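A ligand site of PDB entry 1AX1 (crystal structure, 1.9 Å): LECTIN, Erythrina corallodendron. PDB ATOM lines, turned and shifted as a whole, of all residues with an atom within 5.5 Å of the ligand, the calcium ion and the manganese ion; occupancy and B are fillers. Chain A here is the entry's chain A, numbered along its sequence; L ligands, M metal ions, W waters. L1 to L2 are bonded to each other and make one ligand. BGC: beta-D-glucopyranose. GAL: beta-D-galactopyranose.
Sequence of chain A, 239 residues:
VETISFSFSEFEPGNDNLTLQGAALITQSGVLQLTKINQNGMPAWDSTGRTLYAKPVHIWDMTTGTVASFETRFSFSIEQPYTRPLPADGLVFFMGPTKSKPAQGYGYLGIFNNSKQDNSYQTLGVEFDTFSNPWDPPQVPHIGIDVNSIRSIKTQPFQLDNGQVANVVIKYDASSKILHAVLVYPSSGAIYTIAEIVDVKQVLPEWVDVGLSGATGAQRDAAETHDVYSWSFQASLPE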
ATOM      1  N   PRO A  85      12.482  -8.503 -19.305  1.00  0.00           N
ATOM      2  CA  PRO A  85      11.010  -8.469 -19.337  1.00  0.00           C
ATOM      3  C   PRO A  85      10.491  -9.062 -20.637  1.00  0.00           C
ATOM      4  O   PRO A  85      11.274  -9.467 -21.511  1.00  0.00           O
ATOM      5  CB  PRO A  85      10.713  -6.978 -19.249  1.00  0.00           C
ATOM      6  CG  PRO A  85      11.845  -6.377 -20.002  1.00  0.00           C
ATOM      7  CD  PRO A  85      13.038  -7.152 -19.488  1.00  0.00           C
ATOM      8  N   LEU A  86       9.169  -9.167 -20.753  1.00  0.00           N
ATOM      9  CA  LEU A  86       8.562  -9.704 -21.958  1.00  0.00           C
ATOM     10  C   LEU A  86       8.925  -8.806 -23.145  1.00  0.00           C
ATOM     11  O   LEU A  86       9.006  -7.591 -23.003  1.00  0.00           O
ATOM     12  CB  LEU A  86       7.043  -9.776 -21.807  1.00  0.00           C
ATOM     13  CG  LEU A  86       6.524 -10.634 -20.656  1.00  0.00           C
ATOM     14  CD1 LEU A  86       5.019 -10.517 -20.584  1.00  0.00           C
ATOM     15  CD2 LEU A  86       6.946 -12.080 -20.859  1.00  0.00           C
ATOM     16  N   ALA A  88       8.597  -6.862 -26.885  1.00  0.00           N
ATOM     17  CA  ALA A  88       7.558  -6.024 -27.471  1.00  0.00           C
ATOM     18  C   ALA A  88       8.166  -5.238 -28.632  1.00  0.00           C
ATOM     19  O   ALA A  88       9.383  -5.168 -28.725  1.00  0.00           O
ATOM     20  CB  ALA A  88       7.040  -5.074 -26.405  1.00  0.00           C
ATOM     21  N   ASP A  89       7.358  -4.674 -29.544  1.00  0.00           N
ATOM     22  CA  ASP A  89       5.897  -4.732 -29.539  1.00  0.00           C
ATOM     23  C   ASP A  89       5.341  -5.425 -30.776  1.00  0.00           C
ATOM     24  O   ASP A  89       4.201  -5.911 -30.782  1.00  0.00           O
ATOM     25  CB  ASP A  89       5.297  -3.327 -29.458  1.00  0.00           C
ATOM     26  CG  ASP A  89       5.033  -2.888 -28.037  1.00  0.00           C
ATOM     27  OD1 ASP A  89       4.026  -3.334 -27.456  1.00  0.00           O
ATOM     28  OD2 ASP A  89       5.850  -2.112 -27.503  1.00  0.00           O
ATOM     29  N   TYR A 106       5.244   1.838 -29.390  1.00  0.00           N
ATOM     30  CA  TYR A 106       4.833   0.785 -28.465  1.00  0.00           C
ATOM     31  C   TYR A 106       3.698  -0.062 -29.041  1.00  0.00           C
ATOM     32  O   TYR A 106       3.757  -0.464 -30.210  1.00  0.00           O
ATOM     33  CB  TYR A 106       4.431   1.374 -27.101  1.00  0.00           C
ATOM     34  CG  TYR A 106       5.413   2.386 -26.576  1.00  0.00           C
ATOM     35  CD1 TYR A 106       6.779   2.121 -26.575  1.00  0.00           C
ATOM     36  CD2 TYR A 106       4.981   3.623 -26.111  1.00  0.00           C
ATOM     37  CE1 TYR A 106       7.697   3.078 -26.145  1.00  0.00           C
ATOM     38  CE2 TYR A 106       5.877   4.582 -25.688  1.00  0.00           C
ATOM     39  CZ  TYR A 106       7.229   4.309 -25.702  1.00  0.00           C
ATOM     40  OH  TYR A 106       8.110   5.259 -25.252  1.00  0.00           O
ATOM     41  N   GLY A 107       2.687  -0.346 -28.214  1.00  0.00           N
ATOM     42  CA  GLY A 107       1.553  -1.149 -28.620  1.00  0.00           C
ATOM     43  C   GLY A 107       0.772  -0.603 -29.793  1.00  0.00           C
ATOM     44  O   GLY A 107      -0.034  -1.313 -30.390  1.00  0.00           O
ATOM     45  N   GLU A 127      -1.068  -6.844 -38.653  1.00  0.00           N
ATOM     46  CA  GLU A 127      -0.037  -6.865 -37.629  1.00  0.00           C
ATOM     47  C   GLU A 127       0.487  -8.242 -37.246  1.00  0.00           C
ATOM     48  O   GLU A 127      -0.152  -9.268 -37.465  1.00  0.00           O
ATOM     49  CB  GLU A 127      -0.550  -6.170 -36.376  1.00  0.00           C
ATOM     50  CG  GLU A 127      -1.764  -6.871 -35.768  1.00  0.00           C
ATOM     51  CD  GLU A 127      -2.180  -6.315 -34.425  1.00  0.00           C
ATOM     52  OE1 GLU A 127      -2.304  -5.091 -34.299  1.00  0.00           O
ATOM     53  OE2 GLU A 127      -2.379  -7.123 -33.493  1.00  0.00           O
ATOM     54  N   ASP A 129       1.856  -8.979 -33.908  1.00  0.00           N
ATOM     55  CA  ASP A 129       1.890  -8.498 -32.537  1.00  0.00           C
ATOM     56  C   ASP A 129       2.552  -9.440 -31.536  1.00  0.00           C
ATOM     57  O   ASP A 129       2.055 -10.537 -31.295  1.00  0.00           O
ATOM     58  CB  ASP A 129       0.447  -8.211 -32.124  1.00  0.00           C
ATOM     59  CG  ASP A 129       0.343  -7.283 -30.940  1.00  0.00           C
ATOM     60  OD1 ASP A 129       1.325  -7.084 -30.196  1.00  0.00           O
ATOM     61  OD2 ASP A 129      -0.759  -6.737 -30.747  1.00  0.00           O
ATOM     62  N   THR A 130       3.602  -8.959 -30.890  1.00  0.00           N
ATOM     63  CA  THR A 130       4.350  -9.768 -29.929  1.00  0.00           C
ATOM     64  C   THR A 130       4.104  -9.472 -28.442  1.00  0.00           C
ATOM     65  O   THR A 130       4.620 -10.196 -27.585  1.00  0.00           O
ATOM     66  CB  THR A 130       5.864  -9.693 -30.194  1.00  0.00           C
ATOM     67  OG1 THR A 130       6.310  -8.335 -30.078  1.00  0.00           O
ATOM     68  CG2 THR A 130       6.192 -10.208 -31.597  1.00  0.00           C
ATOM     69  N   PHE A 131       3.352  -8.419 -28.138  1.00  0.00           N
ATOM     70  CA  PHE A 131       3.065  -8.079 -26.746  1.00  0.00           C
ATOM     71  C   PHE A 131       1.572  -7.922 -26.532  1.00  0.00           C
ATOM     72  O   PHE A 131       0.900  -7.213 -27.276  1.00  0.00           O
ATOM     73  CB  PHE A 131       3.794  -6.793 -26.334  1.00  0.00           C
ATOM     74  CG  PHE A 131       3.556  -6.414 -24.897  1.00  0.00           C
ATOM     75  CD1 PHE A 131       2.468  -5.628 -24.535  1.00  0.00           C
ATOM     76  CD2 PHE A 131       4.405  -6.880 -23.891  1.00  0.00           C
ATOM     77  CE1 PHE A 131       2.212  -5.300 -23.212  1.00  0.00           C
ATOM     78  CE2 PHE A 131       4.169  -6.555 -22.560  1.00  0.00           C
ATOM     79  CZ  PHE A 131       3.061  -5.767 -22.220  1.00  0.00           C
ATOM     80  N   SER A 132       1.074  -8.555 -25.481  1.00  0.00           N
ATOM     81  CA  SER A 132      -0.345  -8.511 -25.149  1.00  0.00           C
ATOM     82  C   SER A 132      -0.776  -7.279 -24.330  1.00  0.00           C
ATOM     83  O   SER A 132      -0.557  -7.225 -23.117  1.00  0.00           O
ATOM     84  CB  SER A 132      -0.750  -9.813 -24.449  1.00  0.00           C
ATOM     85  OG  SER A 132      -2.156  -9.936 -24.378  1.00  0.00           O
ATOM     86  N   ASN A 133      -1.341  -6.285 -25.022  1.00  0.00           N
ATOM     87  CA  ASN A 133      -1.841  -5.058 -24.397  1.00  0.00           C
ATOM     88  C   ASN A 133      -3.259  -5.352 -23.900  1.00  0.00           C
ATOM     89  O   ASN A 133      -3.811  -6.410 -24.178  1.00  0.00           O
ATOM     90  CB  ASN A 133      -1.870  -3.918 -25.420  1.00  0.00           C
ATOM     91  CG  ASN A 133      -0.488  -3.560 -25.933  1.00  0.00           C
ATOM     92  OD1 ASN A 133      -0.048  -4.053 -26.963  1.00  0.00           O
ATOM     93  ND2 ASN A 133       0.194  -2.676 -25.222  1.00  0.00           N
ATOM     94  N   TRP A 135      -6.037  -4.360 -24.905  1.00  0.00           N
ATOM     95  CA  TRP A 135      -6.975  -4.505 -26.023  1.00  0.00           C
ATOM     96  C   TRP A 135      -6.700  -5.766 -26.857  1.00  0.00           C
ATOM     97  O   TRP A 135      -7.427  -6.057 -27.808  1.00  0.00           O
ATOM     98  CB  TRP A 135      -6.910  -3.269 -26.929  1.00  0.00           C
ATOM     99  CG  TRP A 135      -5.524  -2.999 -27.449  1.00  0.00           C
ATOM    100  CD1 TRP A 135      -4.864  -3.680 -28.446  1.00  0.00           C
ATOM    101  CD2 TRP A 135      -4.623  -1.980 -26.998  1.00  0.00           C
ATOM    102  NE1 TRP A 135      -3.613  -3.142 -28.641  1.00  0.00           N
ATOM    103  CE2 TRP A 135      -3.441  -2.103 -27.757  1.00  0.00           C
ATOM    104  CE3 TRP A 135      -4.700  -0.991 -26.019  1.00  0.00           C
ATOM    105  CZ2 TRP A 135      -2.330  -1.255 -27.579  1.00  0.00           C
ATOM    106  CZ3 TRP A 135      -3.599  -0.139 -25.827  1.00  0.00           C
ATOM    107  CH2 TRP A 135      -2.436  -0.284 -26.601  1.00  0.00           C
ATOM    108  N   ASP A 136      -5.642  -6.493 -26.519  1.00  0.00           N
ATOM    109  CA  ASP A 136      -5.246  -7.694 -27.241  1.00  0.00           C
ATOM    110  C   ASP A 136      -5.743  -8.991 -26.638  1.00  0.00           C
ATOM    111  O   ASP A 136      -6.134  -9.044 -25.466  1.00  0.00           O
ATOM    112  CB  ASP A 136      -3.723  -7.813 -27.263  1.00  0.00           C
ATOM    113  CG  ASP A 136      -3.080  -6.913 -28.275  1.00  0.00           C
ATOM    114  OD1 ASP A 136      -3.640  -6.788 -29.384  1.00  0.00           O
ATOM    115  OD2 ASP A 136      -2.006  -6.345 -27.968  1.00  0.00           O
ATOM    116  N   PRO A 137      -5.791 -10.065 -27.452  1.00  0.00           N
ATOM    117  CA  PRO A 137      -6.213 -11.349 -26.916  1.00  0.00           C
ATOM    118  C   PRO A 137      -5.015 -11.765 -26.044  1.00  0.00           C
ATOM    119  O   PRO A 137      -3.920 -11.202 -26.189  1.00  0.00           O
ATOM    120  CB  PRO A 137      -6.344 -12.222 -28.175  1.00  0.00           C
ATOM    121  CG  PRO A 137      -5.474 -11.544 -29.181  1.00  0.00           C
ATOM    122  CD  PRO A 137      -5.754 -10.094 -28.923  1.00  0.00           C
ATOM    123  N   HIS A 142       0.557 -12.933 -32.320  1.00  0.00           N
ATOM    124  CA  HIS A 142      -0.646 -13.162 -33.110  1.00  0.00           C
ATOM    125  C   HIS A 142      -0.673 -12.253 -34.329  1.00  0.00           C
ATOM    126  O   HIS A 142      -0.074 -11.174 -34.339  1.00  0.00           O
ATOM    127  CB  HIS A 142      -1.931 -12.992 -32.285  1.00  0.00           C
ATOM    128  CG  HIS A 142      -2.117 -11.613 -31.703  1.00  0.00           C
ATOM    129  ND1 HIS A 142      -1.810 -11.288 -30.403  1.00  0.00           N
ATOM    130  CD2 HIS A 142      -2.589 -10.476 -32.265  1.00  0.00           C
ATOM    131  CE1 HIS A 142      -2.101  -9.988 -30.215  1.00  0.00           C
ATOM    132  NE2 HIS A 142      -2.574  -9.459 -31.317  1.00  0.00           N
ATOM    133  N   ILE A 150      -6.332  -0.353 -33.425  1.00  0.00           N
ATOM    134  CA  ILE A 150      -5.300  -1.294 -33.009  1.00  0.00           C
ATOM    135  C   ILE A 150      -5.988  -2.557 -32.450  1.00  0.00           C
ATOM    136  O   ILE A 150      -5.368  -3.609 -32.299  1.00  0.00           O
ATOM    137  CB  ILE A 150      -4.326  -0.651 -31.965  1.00  0.00           C
ATOM    138  CG1 ILE A 150      -3.087  -1.529 -31.781  1.00  0.00           C
ATOM    139  CG2 ILE A 150      -5.043  -0.368 -30.655  1.00  0.00           C
ATOM    140  CD1 ILE A 150      -2.197  -1.621 -33.021  1.00  0.00           C
ATOM    141  N   SER A 152      -7.794  -5.381 -33.266  1.00  0.00           N
ATOM    142  CA  SER A 152      -8.077  -6.170 -34.462  1.00  0.00           C
ATOM    143  C   SER A 152      -9.502  -6.687 -34.572  1.00  0.00           C
ATOM    144  O   SER A 152     -10.128  -7.003 -33.565  1.00  0.00           O
ATOM    145  CB  SER A 152      -7.129  -7.370 -34.522  1.00  0.00           C
ATOM    146  OG  SER A 152      -5.801  -6.957 -34.323  1.00  0.00           O
ATOM    147  N   THR A 155      -8.184 -12.085 -35.190  1.00  0.00           N
ATOM    148  CA  THR A 155      -6.858 -12.431 -34.680  1.00  0.00           C
ATOM    149  C   THR A 155      -6.517 -13.910 -34.893  1.00  0.00           C
ATOM    150  O   THR A 155      -7.408 -14.768 -34.920  1.00  0.00           O
ATOM    151  CB  THR A 155      -6.755 -12.023 -33.171  1.00  0.00           C
ATOM    152  OG1 THR A 155      -6.055 -10.782 -33.057  1.00  0.00           O
ATOM    153  CG2 THR A 155      -6.091 -13.073 -32.339  1.00  0.00           C
ATOM    154  N   THR A 216       9.505  -1.166 -30.565  1.00  0.00           N
ATOM    155  CA  THR A 216       9.967  -1.900 -29.384  1.00  0.00           C
ATOM    156  C   THR A 216       9.275  -1.285 -28.146  1.00  0.00           C
ATOM    157  O   THR A 216       8.675  -0.205 -28.232  1.00  0.00           O
ATOM    158  CB  THR A 216      11.506  -1.943 -29.242  1.00  0.00           C
ATOM    159  OG1 THR A 216      12.052  -0.621 -29.271  1.00  0.00           O
ATOM    160  CG2 THR A 216      12.096  -2.769 -30.377  1.00  0.00           C
ATOM    161  N   GLY A 217       9.347  -1.987 -27.019  1.00  0.00           N
ATOM    162  CA  GLY A 217       8.678  -1.585 -25.793  1.00  0.00           C
ATOM    163  C   GLY A 217       8.945  -0.285 -25.055  1.00  0.00           C
ATOM    164  O   GLY A 217       9.931   0.416 -25.299  1.00  0.00           O
ATOM    165  N   ALA A 218       8.057  -0.027 -24.093  1.00  0.00           N
ATOM    166  CA  ALA A 218       8.075   1.176 -23.245  1.00  0.00           C
ATOM    167  C   ALA A 218       8.975   1.134 -22.000  1.00  0.00           C
ATOM    168  O   ALA A 218       9.049   2.111 -21.262  1.00  0.00           O
ATOM    169  CB  ALA A 218       6.653   1.531 -22.846  1.00  0.00           C
ATOM    170  N   GLN A 219       9.633   0.009 -21.742  1.00  0.00           N
ATOM    171  CA  GLN A 219      10.530  -0.100 -20.588  1.00  0.00           C
ATOM    172  C   GLN A 219      11.836  -0.776 -20.990  1.00  0.00           C
ATOM    173  O   GLN A 219      11.888  -1.488 -22.001  1.00  0.00           O
ATOM    174  CB  GLN A 219       9.867  -0.837 -19.423  1.00  0.00           C
ATOM    175  CG  GLN A 219       9.722  -2.318 -19.637  1.00  0.00           C
ATOM    176  CD  GLN A 219       9.146  -3.002 -18.412  1.00  0.00           C
ATOM    177  OE1 GLN A 219       9.845  -3.731 -17.716  1.00  0.00           O
ATOM    178  NE2 GLN A 219       7.862  -2.771 -18.161  1.00  0.00           N
ATOM    179  N   ALA A 222      12.575  -4.308 -23.002  1.00  0.00           N
ATOM    180  CA  ALA A 222      11.354  -4.906 -23.534  1.00  0.00           C
ATOM    181  C   ALA A 222      11.529  -4.640 -25.029  1.00  0.00           C
ATOM    182  O   ALA A 222      11.002  -3.666 -25.563  1.00  0.00           O
ATOM    183  CB  ALA A 222      10.110  -4.198 -22.988  1.00  0.00           C
HETATM  184  C2  BGC L   1       5.710   0.440 -17.981  1.00  0.00           C
HETATM  185  C3  BGC L   1       5.565   0.277 -19.487  1.00  0.00           C
HETATM  186  C4  BGC L   1       4.090   0.145 -19.872  1.00  0.00           C
HETATM  187  C5  BGC L   1       3.299   1.313 -19.281  1.00  0.00           C
HETATM  188  C6  BGC L   1       1.808   1.233 -19.539  1.00  0.00           C
HETATM  189  C1  BGC L   1       4.843   1.598 -17.507  1.00  0.00           C
HETATM  190  O1  BGC L   1       4.903   1.685 -16.124  1.00  0.00           O
HETATM  191  O2  BGC L   1       7.072   0.679 -17.652  1.00  0.00           O
HETATM  192  O3  BGC L   1       6.288  -0.877 -19.898  1.00  0.00           O
HETATM  193  O4  BGC L   1       3.947   0.183 -21.309  1.00  0.00           O
HETATM  194  O5  BGC L   1       3.475   1.369 -17.857  1.00  0.00           O
HETATM  195  O6  BGC L   1       1.337  -0.108 -19.422  1.00  0.00           O
HETATM  196  C1  GAL L   2       3.860  -1.030 -21.982  1.00  0.00           C
HETATM  197  C2  GAL L   2       3.331  -0.752 -23.396  1.00  0.00           C
HETATM  198  C3  GAL L   2       3.389  -2.030 -24.247  1.00  0.00           C
HETATM  199  C4  GAL L   2       4.830  -2.563 -24.240  1.00  0.00           C
HETATM  200  C5  GAL L   2       5.227  -2.811 -22.790  1.00  0.00           C
HETATM  201  C6  GAL L   2       6.632  -3.360 -22.658  1.00  0.00           C
HETATM  202  O2  GAL L   2       1.993  -0.276 -23.334  1.00  0.00           O
HETATM  203  O3  GAL L   2       2.992  -1.744 -25.577  1.00  0.00           O
HETATM  204  O4  GAL L   2       5.703  -1.619 -24.831  1.00  0.00           O
HETATM  205  O5  GAL L   2       5.187  -1.579 -22.045  1.00  0.00           O
HETATM  206  O6  GAL L   2       6.952  -3.572 -21.296  1.00  0.00           O
HETATM  207 CA    CA M   1       0.115  -5.586 -28.741  1.00  0.00          CA
HETATM  208 MN    MN M   2      -2.796  -7.176 -31.360  1.00  0.00          MN
HETATM  209  O   HOH W   1       2.177  -4.721 -28.902  1.00  0.00           O
HETATM  210  O   HOH W   2       7.888  -5.971 -20.937  1.00  0.00           O
HETATM  211  O   HOH W   3      -3.084  -4.803 -31.669  1.00  0.00           O
HETATM  212  O   HOH W   4      -0.885  -3.877 -30.004  1.00  0.00           O
HETATM  213  O   HOH W   5      -4.868  -7.537 -31.862  1.00  0.00           O
HETATM  214  O   HOH W   6       1.021   0.907 -25.837  1.00  0.00           O
HETATM  215  O   HOH W   7       1.797   2.869 -23.425  1.00  0.00           O
HETATM  216  O   HOH W   8       0.755  -3.145 -20.429  1.00  0.00           O
HETATM  217  O   HOH W   9      -0.360  -1.583 -22.524  1.00  0.00           O
HETATM  218  O   HOH W  10       8.809   2.761 -18.362  1.00  0.00           O
HETATM  219  O   HOH W  11       4.663  -4.365 -19.200  1.00  0.00           O
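An oxygen (O3) of GAL L2 is in hydrogen-bond range of the side-chain amide nitrogen (ND2) of Asn 133 (3.0 Å).
OD1 of Asp 89 sits at hydrogen-bond distance from O3 of GAL L2 (2.7 Å).
The backbone NH (N) of Ala 218 is in hydrogen-bond range of an oxygen (O4) of GAL L2 (2.9 Å).
The backbone NH of Gly 107 sits at hydrogen-bond distance from an oxygen (O3) of GAL L2 (3.0 Å).
An oxygen (O3) of BGC L1 lies within hydrogen-bond range of the side-chain amide nitrogen (NE2) of Gln 219 (3.0 Å).
The backbone NH (N) of Gly 107 is in hydrogen-bond range of the side-chain carboxylate (OD1) of Asp 89, at 3.4 Å.
N of Thr 130 is in hydrogen-bond range of O of Asp 89, 3.1 Å away.
O of Ala 222 lies within hydrogen-bond range of N of Gly 217 (2.8 Å).
Merely in contact with the ligand: Gly 217, Ala 222, Tyr 106 and Ala 88.
Hydrophobic or aromatic side chains within 4 Å of the ligand: Ala 88, Tyr 106, Phe 131, Ala 218 and Ala 222.
Ten residues have an atom within 4 Å of the ligand: Ala 88, Asp 89, Tyr 106, Gly 107, Phe 131, Asn 133, Gly 217, Ala 218, Gln 219 and Ala 222.
Along chain A the residues within 4 Å of the ligand span positions 88 to 222.
Within 4 Å of the calcium ion: Asp 129, Phe 131, Asn 133 and Asp 136.
The nearest printed residue that does not touch the calcium ion is Trp 135 (4.5 Å).
Of the 24 residues printed, 4 come within 4 Å of the manganese ion.
The calcium ion is bound by water W1 (2.2 Å), the backbone carbonyl oxygen (O) of Phe 131 (2.3 Å), water W4 (2.3 Å), the side-chain amide oxygen (OD1) of Asn 133 (2.4 Å), the side-chain carboxylate (OD2) of Asp 136 (2.4 Å), the side-chain carboxylate (OD1) of Asp 129 (2.4 Å) and the side-chain carboxylate (OD2) of Asp 129 (2.5 Å).
The calcium ion has seven donor atoms within binding distance.
The manganese ion is bound by water W5 (2.2 Å).
OD2 of Asp 129 is bound to the manganese ion (2.2 Å).
The manganese ion is bound by the side-chain carboxylate (OE2) of Glu 127 (2.2 Å).
The side-chain carboxylate (OD1) of Asp 136 binds the manganese ion.
The manganese ion is bound by NE2 of His 142 (2.3 Å).
The manganese ion is bound by water W3 (2.4 Å).
Water W4 lies within hydrogen-bond range of the backbone carbonyl oxygen of Gly 107 (2.7 Å) and the indole nitrogen of Trp 135 (3.1 Å).
Water W3 lies within hydrogen-bond range of the backbone carbonyl oxygen (O) of Ile 150 (2.7 Å), the side-chain carboxylate (OE1) of Glu 127 (2.8 Å) and the indole nitrogen (NE1) of Trp 135 (3.5 Å).
Water W2 bridges an oxygen (O6) of GAL L2 (2.6 Å) and the backbone carbonyl oxygen (O) of Leu 86 (2.9 Å).
Water W10 lies within hydrogen-bond range of O2 of BGC L1 and O of Ala 218.
Water W9 bridges an oxygen (O2) of GAL L2 and the side-chain amide nitrogen (ND2) of Asn 133.
Water W6 lies within hydrogen-bond range of O2 of GAL L2 (2.9 Å) and N of Gly 107 (3.2 Å).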
